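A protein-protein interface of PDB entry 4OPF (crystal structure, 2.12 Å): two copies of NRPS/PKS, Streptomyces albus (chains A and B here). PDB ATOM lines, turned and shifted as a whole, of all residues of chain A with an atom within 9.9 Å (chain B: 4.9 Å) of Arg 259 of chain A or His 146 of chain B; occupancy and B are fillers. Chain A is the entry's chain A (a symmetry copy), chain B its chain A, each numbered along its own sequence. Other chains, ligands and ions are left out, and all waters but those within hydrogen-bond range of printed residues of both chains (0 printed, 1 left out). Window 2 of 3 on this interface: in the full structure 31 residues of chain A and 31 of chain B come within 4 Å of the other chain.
O of His 145 of chain B is in hydrogen-bond range of NE of Arg 259 of chain A, 3.2 Å away.
NE2 of His 145 of chain B is in hydrogen-bond range of O of Thr 260 of chain A, at 3.2 Å.
The guanidinium group (NH2) of Arg 259 of chain A is in hydrogen-bond range of the backbone carbonyl oxygen (O) of His 146 of chain B.
The side-chain carboxylate of Asp 148 of chain B lies within hydrogen-bond range of the backbone NH of Arg 259 of chain A (2.8 Å).
OD1 of Asn 256 of chain A sits at hydrogen-bond distance from N of Gly 258 of chain A (2.8 Å).
O of Gly 262 of chain A sits at hydrogen-bond distance from OG1 of Thr 260 of chain A.
Asn 256 of chain A touches Ser 144 of chain B.
Ser 144 of chain B touches Gly 258 of chain A.
Gly 258 of chain A touches His 145 of chain B (O to CA, 3.8 Å).
Asp 148 of chain B touches Gly 258 of chain A (OD1 to CA, 3.4 Å).
Arg 259 of chain A touches just these residues of chain B: His 145, His 146 and Asp 148.
His 146 of chain B touches one residue of chain A.
Of the printed residues of chain A, His 145 of chain B touches Gly 258 (3.8 Å), Arg 259 (3.2 Å) and Thr 260 (3.2 Å).
No residue of chain A comes within 4 Å of Phe 147 of chain B.
Of the printed residues of chain A, Ser 144 of chain B touches Asn 256 (3.6 Å) and Gly 258 (3.7 Å).
Of the printed residues of chain B, Gly 258 of chain A touches Ser 144, His 145 and Asp 148.
Of the printed residues of chain B, Thr 260 of chain A touches His 145.
Pro 268 of chain A touches none of the printed residues of chain B.
Asn 142 of chain B touches none of the printed residues of chain A.
The nearest residue of chain B that does not touch Arg 259 of chain A is His 68 of chain B (4.02 Å).
The nearest residue of chain A that does not touch His 146 of chain B is Gly 258 of chain A (5.9 Å).
The nearest printed residue of chain A that does not touch Ser 144 of chain B is Arg 259 of chain A (4.1 Å).
Of the 17 printed residues of chain A, 4 touch a printed residue of chain B.
Among the printed residues, no Asp or Glu carboxylate lies within 4 Å of a Lys or Arg side-chain nitrogen of the other chain.
No position is printed for both chains.
Of the 8 pairs that touch across the chains among the printed residues, none has its exchanged pair printed and touching as well.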
ATOM      1  N   ASN A 256     -20.927  -0.671 -15.138  1.00  0.00           N
ATOM      2  CA  ASN A 256     -19.805  -0.094 -14.424  1.00  0.00           C
ATOM      3  C   ASN A 256     -19.997  -0.325 -12.933  1.00  0.00           C
ATOM      4  O   ASN A 256     -21.103  -0.202 -12.415  1.00  0.00           O
ATOM      5  CB  ASN A 256     -19.751   1.420 -14.635  1.00  0.00           C
ATOM      6  CG  ASN A 256     -18.401   1.985 -14.316  1.00  0.00           C
ATOM      7  OD1 ASN A 256     -18.167   2.463 -13.228  1.00  0.00           O
ATOM      8  ND2 ASN A 256     -17.495   1.922 -15.274  1.00  0.00           N
ATOM      9  N   ASP A 257     -18.888  -0.558 -12.232  1.00  0.00           N
ATOM     10  CA  ASP A 257     -18.913  -0.683 -10.791  1.00  0.00           C
ATOM     11  C   ASP A 257     -19.390   0.575 -10.072  1.00  0.00           C
ATOM     12  O   ASP A 257     -19.762   0.539  -8.894  1.00  0.00           O
ATOM     13  CB  ASP A 257     -17.504  -0.938 -10.287  1.00  0.00           C
ATOM     14  CG  ASP A 257     -17.025  -2.318 -10.571  1.00  0.00           C
ATOM     15  OD1 ASP A 257     -17.869  -3.209 -10.784  1.00  0.00           O
ATOM     16  OD2 ASP A 257     -15.774  -2.497 -10.577  1.00  0.00           O
ATOM     17  N   GLY A 258     -19.236   1.734 -10.692  1.00  0.00           N
ATOM     18  CA  GLY A 258     -19.570   2.957  -9.948  1.00  0.00           C
ATOM     19  C   GLY A 258     -18.537   3.339  -8.887  1.00  0.00           C
ATOM     20  O   GLY A 258     -17.356   3.203  -9.093  1.00  0.00           O
ATOM     21  N   ARG A 259     -18.986   3.839  -7.781  1.00  0.00           N
ATOM     22  CA  ARG A 259     -18.126   4.364  -6.768  1.00  0.00           C
ATOM     23  C   ARG A 259     -17.617   3.191  -5.913  1.00  0.00           C
ATOM     24  O   ARG A 259     -18.404   2.565  -5.215  1.00  0.00           O
ATOM     25  CB  ARG A 259     -18.958   5.259  -5.901  1.00  0.00           C
ATOM     26  CG  ARG A 259     -18.308   5.636  -4.596  1.00  0.00           C
ATOM     27  CD  ARG A 259     -17.377   6.782  -4.770  1.00  0.00           C
ATOM     28  NE  ARG A 259     -18.096   8.031  -4.951  1.00  0.00           N
ATOM     29  CZ  ARG A 259     -18.472   8.867  -3.990  1.00  0.00           C
ATOM     30  NH1 ARG A 259     -18.239   8.601  -2.709  1.00  0.00           N
ATOM     31  NH2 ARG A 259     -19.092   9.998  -4.309  1.00  0.00           N
ATOM     32  N   THR A 260     -16.349   2.862  -5.982  1.00  0.00           N
ATOM     33  CA  THR A 260     -15.802   1.787  -5.120  1.00  0.00           C
ATOM     34  C   THR A 260     -14.690   2.388  -4.221  1.00  0.00           C
ATOM     35  O   THR A 260     -14.192   3.498  -4.485  1.00  0.00           O
ATOM     36  CB  THR A 260     -15.182   0.633  -5.952  1.00  0.00           C
ATOM     37  OG1 THR A 260     -14.271   1.196  -6.910  1.00  0.00           O
ATOM     38  CG2 THR A 260     -16.273  -0.244  -6.658  1.00  0.00           C
ATOM     39  N   ALA A 261     -14.284   1.648  -3.184  1.00  0.00           N
ATOM     40  CA  ALA A 261     -13.227   2.127  -2.276  1.00  0.00           C
ATOM     41  C   ALA A 261     -11.888   2.389  -2.989  1.00  0.00           C
ATOM     42  O   ALA A 261     -11.141   3.265  -2.590  1.00  0.00           O
ATOM     43  CB  ALA A 261     -13.045   1.162  -1.129  1.00  0.00           C
ATOM     44  N   GLY A 262     -11.597   1.659  -4.057  1.00  0.00           N
ATOM     45  CA  GLY A 262     -10.397   1.918  -4.813  1.00  0.00           C
ATOM     46  C   GLY A 262     -10.369   1.106  -6.081  1.00  0.00           C
ATOM     47  O   GLY A 262     -11.412   0.635  -6.545  1.00  0.00           O
ATOM     48  N   PRO A 263      -9.166   0.907  -6.637  1.00  0.00           N
ATOM     49  CA  PRO A 263      -9.062   0.360  -7.995  1.00  0.00           C
ATOM     50  C   PRO A 263      -9.351  -1.151  -8.101  1.00  0.00           C
ATOM     51  O   PRO A 263     -10.155  -1.559  -8.941  1.00  0.00           O
ATOM     52  CB  PRO A 263      -7.615   0.706  -8.412  1.00  0.00           C
ATOM     53  CG  PRO A 263      -6.894   1.145  -7.157  1.00  0.00           C
ATOM     54  CD  PRO A 263      -7.848   1.110  -5.997  1.00  0.00           C
ATOM     55  N   THR A 265     -11.027  -3.012  -6.075  1.00  0.00           N
ATOM     56  CA  THR A 265     -12.160  -3.343  -5.203  1.00  0.00           C
ATOM     57  C   THR A 265     -13.368  -3.610  -6.093  1.00  0.00           C
ATOM     58  O   THR A 265     -13.912  -2.709  -6.716  1.00  0.00           O
ATOM     59  CB  THR A 265     -12.438  -2.243  -4.174  1.00  0.00           C
ATOM     60  OG1 THR A 265     -11.219  -1.956  -3.492  1.00  0.00           O
ATOM     61  CG2 THR A 265     -13.502  -2.697  -3.152  1.00  0.00           C
ATOM     62  N   PRO A 266     -13.747  -4.865  -6.201  1.00  0.00           N
ATOM     63  CA  PRO A 266     -14.881  -5.256  -7.010  1.00  0.00           C
ATOM     64  C   PRO A 266     -16.216  -4.811  -6.377  1.00  0.00           C
ATOM     65  O   PRO A 266     -16.270  -4.510  -5.189  1.00  0.00           O
ATOM     66  CB  PRO A 266     -14.786  -6.794  -7.038  1.00  0.00           C
ATOM     67  CG  PRO A 266     -13.461  -7.110  -6.462  1.00  0.00           C
ATOM     68  CD  PRO A 266     -13.146  -6.011  -5.507  1.00  0.00           C
ATOM     69  N   ASN A 267     -17.252  -4.699  -7.204  1.00  0.00           N
ATOM     70  CA  ASN A 267     -18.600  -4.391  -6.750  1.00  0.00           C
ATOM     71  C   ASN A 267     -19.378  -5.654  -7.081  1.00  0.00           C
ATOM     72  O   ASN A 267     -19.711  -5.890  -8.214  1.00  0.00           O
ATOM     73  CB  ASN A 267     -19.168  -3.190  -7.502  1.00  0.00           C
ATOM     74  CG  ASN A 267     -20.577  -2.882  -7.103  1.00  0.00           C
ATOM     75  OD1 ASN A 267     -21.242  -3.718  -6.523  1.00  0.00           O
ATOM     76  ND2 ASN A 267     -21.048  -1.676  -7.400  1.00  0.00           N
ATOM     77  N   PRO A 268     -19.586  -6.515  -6.110  1.00  0.00           N
ATOM     78  CA  PRO A 268     -20.300  -7.750  -6.329  1.00  0.00           C
ATOM     79  C   PRO A 268     -21.664  -7.537  -6.970  1.00  0.00           C
ATOM     80  O   PRO A 268     -22.058  -8.283  -7.851  1.00  0.00           O
ATOM     81  CB  PRO A 268     -20.469  -8.313  -4.907  1.00  0.00           C
ATOM     82  CG  PRO A 268     -19.291  -7.742  -4.140  1.00  0.00           C
ATOM     83  CD  PRO A 268     -19.108  -6.363  -4.713  1.00  0.00           C
ATOM     84  N   ALA A 269     -22.388  -6.517  -6.571  1.00  0.00           N
ATOM     85  CA  ALA A 269     -23.751  -6.261  -7.142  1.00  0.00           C
ATOM     86  C   ALA A 269     -23.677  -5.949  -8.646  1.00  0.00           C
ATOM     87  O   ALA A 269     -24.561  -6.336  -9.424  1.00  0.00           O
ATOM     88  CB  ALA A 269     -24.405  -5.132  -6.376  1.00  0.00           C
ATOM     89  N   ALA A 270     -22.590  -5.287  -9.082  1.00  0.00           N
ATOM     90  CA  ALA A 270     -22.434  -4.947 -10.493  1.00  0.00           C
ATOM     91  C   ALA A 270     -22.071  -6.198 -11.283  1.00  0.00           C
ATOM     92  O   ALA A 270     -22.514  -6.377 -12.385  1.00  0.00           O
ATOM     93  CB  ALA A 270     -21.353  -3.892 -10.669  1.00  0.00           C
ATOM     94  N   ASP A 398     -10.441  -3.924 -13.694  1.00  0.00           N
ATOM     95  CA  ASP A 398     -10.095  -3.045 -12.566  1.00  0.00           C
ATOM     96  C   ASP A 398     -10.596  -1.602 -12.691  1.00  0.00           C
ATOM     97  O   ASP A 398     -11.152  -1.059 -11.724  1.00  0.00           O
ATOM     98  CB  ASP A 398      -8.574  -3.064 -12.316  1.00  0.00           C
ATOM     99  CG  ASP A 398      -8.135  -4.276 -11.476  1.00  0.00           C
ATOM    100  OD1 ASP A 398      -9.009  -4.954 -10.862  1.00  0.00           O
ATOM    101  OD2 ASP A 398      -6.910  -4.543 -11.444  1.00  0.00           O
ATOM    102  N   GLY A 399     -10.435  -1.010 -13.872  1.00  0.00           N
ATOM    103  CA  GLY A 399     -11.080   0.284 -14.185  1.00  0.00           C
ATOM    104  C   GLY A 399     -12.566   0.515 -13.819  1.00  0.00           C
ATOM    105  O   GLY A 399     -12.981   1.638 -13.684  1.00  0.00           O
ATOM    106  N   GLY A 400     -13.382  -0.510 -13.633  1.00  0.00           N
ATOM    107  CA  GLY A 400     -14.787  -0.271 -13.278  1.00  0.00           C
ATOM    108  C   GLY A 400     -15.711  -0.955 -14.246  1.00  0.00           C
ATOM    109  O   GLY A 400     -16.832  -1.275 -13.906  1.00  0.00           O
ATOM    110  N   HIS B  66     -14.781  19.529  -3.066  1.00  0.00           N
ATOM    111  CA  HIS B  66     -16.173  19.260  -3.331  1.00  0.00           C
ATOM    112  C   HIS B  66     -16.311  17.914  -3.963  1.00  0.00           C
ATOM    113  O   HIS B  66     -17.267  17.187  -3.712  1.00  0.00           O
ATOM    114  CB  HIS B  66     -16.761  20.323  -4.222  1.00  0.00           C
ATOM    115  CG  HIS B  66     -18.254  20.313  -4.247  1.00  0.00           C
ATOM    116  ND1 HIS B  66     -19.011  21.167  -3.472  1.00  0.00           N
ATOM    117  CD2 HIS B  66     -19.130  19.543  -4.938  1.00  0.00           C
ATOM    118  CE1 HIS B  66     -20.292  20.935  -3.701  1.00  0.00           C
ATOM    119  NE2 HIS B  66     -20.392  19.948  -4.578  1.00  0.00           N
ATOM    120  N   PHE B  67     -15.316  17.525  -4.735  1.00  0.00           N
ATOM    121  CA  PHE B  67     -15.337  16.208  -5.364  1.00  0.00           C
ATOM    122  C   PHE B  67     -14.560  15.137  -4.639  1.00  0.00           C
ATOM    123  O   PHE B  67     -14.215  14.107  -5.247  1.00  0.00           O
ATOM    124  CB  PHE B  67     -14.895  16.364  -6.848  1.00  0.00           C
ATOM    125  CG  PHE B  67     -15.801  17.280  -7.617  1.00  0.00           C
ATOM    126  CD1 PHE B  67     -16.962  16.789  -8.156  1.00  0.00           C
ATOM    127  CD2 PHE B  67     -15.573  18.641  -7.658  1.00  0.00           C
ATOM    128  CE1 PHE B  67     -17.839  17.650  -8.798  1.00  0.00           C
ATOM    129  CE2 PHE B  67     -16.453  19.506  -8.258  1.00  0.00           C
ATOM    130  CZ  PHE B  67     -17.590  19.002  -8.858  1.00  0.00           C
ATOM    131  N   HIS B  68     -14.277  15.339  -3.350  1.00  0.00           N
ATOM    132  CA  HIS B  68     -13.531  14.334  -2.590  1.00  0.00           C
ATOM    133  C   HIS B  68     -12.195  14.028  -3.167  1.00  0.00           C
ATOM    134  O   HIS B  68     -11.710  12.899  -3.127  1.00  0.00           O
ATOM    135  CB  HIS B  68     -14.364  13.040  -2.384  1.00  0.00           C
ATOM    136  CG  HIS B  68     -15.744  13.323  -1.890  1.00  0.00           C
ATOM    137  ND1 HIS B  68     -16.881  12.840  -2.517  1.00  0.00           N
ATOM    138  CD2 HIS B  68     -16.175  14.141  -0.896  1.00  0.00           C
ATOM    139  CE1 HIS B  68     -17.948  13.303  -1.884  1.00  0.00           C
ATOM    140  NE2 HIS B  68     -17.546  14.105  -0.906  1.00  0.00           N
ATOM    141  N   LEU B  85     -16.121  17.061 -14.308  1.00  0.00           N
ATOM    142  CA  LEU B  85     -16.797  16.849 -13.021  1.00  0.00           C
ATOM    143  C   LEU B  85     -17.715  18.045 -12.650  1.00  0.00           C
ATOM    144  O   LEU B  85     -18.873  17.855 -12.272  1.00  0.00           O
ATOM    145  CB  LEU B  85     -15.773  16.623 -11.886  1.00  0.00           C
ATOM    146  CG  LEU B  85     -15.145  15.223 -11.899  1.00  0.00           C
ATOM    147  CD1 LEU B  85     -13.939  15.187 -10.984  1.00  0.00           C
ATOM    148  CD2 LEU B  85     -16.160  14.211 -11.398  1.00  0.00           C
ATOM    149  N   ALA B 141     -14.681   7.408 -16.764  1.00  0.00           N
ATOM    150  CA  ALA B 141     -14.624   6.613 -15.497  1.00  0.00           C
ATOM    151  C   ALA B 141     -14.605   7.502 -14.269  1.00  0.00           C
ATOM    152  O   ALA B 141     -15.209   7.129 -13.267  1.00  0.00           O
ATOM    153  CB  ALA B 141     -13.401   5.679 -15.434  1.00  0.00           C
ATOM    154  N   ASN B 142     -13.962   8.666 -14.334  1.00  0.00           N
ATOM    155  CA  ASN B 142     -14.036   9.587 -13.211  1.00  0.00           C
ATOM    156  C   ASN B 142     -15.431  10.001 -12.897  1.00  0.00           C
ATOM    157  O   ASN B 142     -15.761  10.151 -11.759  1.00  0.00           O
ATOM    158  CB  ASN B 142     -13.275  10.860 -13.478  1.00  0.00           C
ATOM    159  CG  ASN B 142     -11.825  10.692 -13.241  1.00  0.00           C
ATOM    160  OD1 ASN B 142     -11.437  10.137 -12.234  1.00  0.00           O
ATOM    161  ND2 ASN B 142     -11.006  11.178 -14.151  1.00  0.00           N
ATOM    162  N   LEU B 143     -16.261  10.179 -13.923  1.00  0.00           N
ATOM    163  CA  LEU B 143     -17.605  10.612 -13.704  1.00  0.00           C
ATOM    164  C   LEU B 143     -18.415   9.492 -13.090  1.00  0.00           C
ATOM    165  O   LEU B 143     -19.181   9.697 -12.147  1.00  0.00           O
ATOM    166  CB  LEU B 143     -18.257  11.106 -14.997  1.00  0.00           C
ATOM    167  CG  LEU B 143     -17.566  12.242 -15.726  1.00  0.00           C
ATOM    168  CD1 LEU B 143     -18.298  12.650 -16.983  1.00  0.00           C
ATOM    169  CD2 LEU B 143     -17.458  13.435 -14.836  1.00  0.00           C
ATOM    170  N   SER B 144     -18.270   8.304 -13.650  1.00  0.00           N
ATOM    171  CA  SER B 144     -18.993   7.146 -13.151  1.00  0.00           C
ATOM    172  C   SER B 144     -18.590   6.889 -11.711  1.00  0.00           C
ATOM    173  O   SER B 144     -19.445   6.515 -10.901  1.00  0.00           O
ATOM    174  CB  SER B 144     -18.688   5.918 -13.988  1.00  0.00           C
ATOM    175  OG  SER B 144     -19.154   6.110 -15.322  1.00  0.00           O
ATOM    176  N   HIS B 145     -17.313   7.037 -11.401  1.00  0.00           N
ATOM    177  CA  HIS B 145     -16.846   6.794 -10.052  1.00  0.00           C
ATOM    178  C   HIS B 145     -17.391   7.854  -9.083  1.00  0.00           C
ATOM    179  O   HIS B 145     -17.996   7.514  -8.079  1.00  0.00           O
ATOM    180  CB  HIS B 145     -15.313   6.771  -9.999  1.00  0.00           C
ATOM    181  CG  HIS B 145     -14.770   6.578  -8.628  1.00  0.00           C
ATOM    182  ND1 HIS B 145     -14.343   7.621  -7.841  1.00  0.00           N
ATOM    183  CD2 HIS B 145     -14.597   5.455  -7.889  1.00  0.00           C
ATOM    184  CE1 HIS B 145     -13.916   7.153  -6.682  1.00  0.00           C
ATOM    185  NE2 HIS B 145     -14.072   5.841  -6.688  1.00  0.00           N
ATOM    186  N   HIS B 146     -17.258   9.129  -9.427  1.00  0.00           N
ATOM    187  CA  HIS B 146     -17.620  10.166  -8.503  1.00  0.00           C
ATOM    188  C   HIS B 146     -19.123  10.229  -8.258  1.00  0.00           C
ATOM    189  O   HIS B 146     -19.517  10.408  -7.138  1.00  0.00           O
ATOM    190  CB  HIS B 146     -17.156  11.553  -8.912  1.00  0.00           C
ATOM    191  CG  HIS B 146     -17.747  12.619  -8.027  1.00  0.00           C
ATOM    192  ND1 HIS B 146     -17.303  12.851  -6.727  1.00  0.00           N
ATOM    193  CD2 HIS B 146     -18.829  13.425  -8.199  1.00  0.00           C
ATOM    194  CE1 HIS B 146     -18.054  13.792  -6.172  1.00  0.00           C
ATOM    195  NE2 HIS B 146     -18.994  14.148  -7.037  1.00  0.00           N
ATOM    196  N   PHE B 147     -19.950  10.087  -9.295  1.00  0.00           N
ATOM    197  CA  PHE B 147     -21.379  10.162  -9.147  1.00  0.00           C
ATOM    198  C   PHE B 147     -22.031   8.802  -8.919  1.00  0.00           C
ATOM    199  O   PHE B 147     -23.248   8.736  -8.757  1.00  0.00           O
ATOM    200  CB  PHE B 147     -21.945  10.840 -10.388  1.00  0.00           C
ATOM    201  CG  PHE B 147     -21.552  12.287 -10.518  1.00  0.00           C
ATOM    202  CD1 PHE B 147     -22.131  13.244  -9.684  1.00  0.00           C
ATOM    203  CD2 PHE B 147     -20.621  12.698 -11.438  1.00  0.00           C
ATOM    204  CE1 PHE B 147     -21.798  14.591  -9.800  1.00  0.00           C
ATOM    205  CE2 PHE B 147     -20.314  14.039 -11.575  1.00  0.00           C
ATOM    206  CZ  PHE B 147     -20.906  14.982 -10.754  1.00  0.00           C
ATOM    207  N   ASP B 148     -21.220   7.736  -8.875  1.00  0.00           N
ATOM    208  CA  ASP B 148     -21.659   6.326  -8.661  1.00  0.00           C
ATOM    209  C   ASP B 148     -22.718   5.875  -9.726  1.00  0.00           C
ATOM    210  O   ASP B 148     -23.796   5.389  -9.396  1.00  0.00           O
ATOM    211  CB  ASP B 148     -22.223   6.164  -7.282  1.00  0.00           C
ATOM    212  CG  ASP B 148     -22.403   4.700  -6.874  1.00  0.00           C
ATOM    213  OD1 ASP B 148     -21.750   3.727  -7.411  1.00  0.00           O
ATOM    214  OD2 ASP B 148     -23.178   4.529  -5.923  1.00  0.00           O
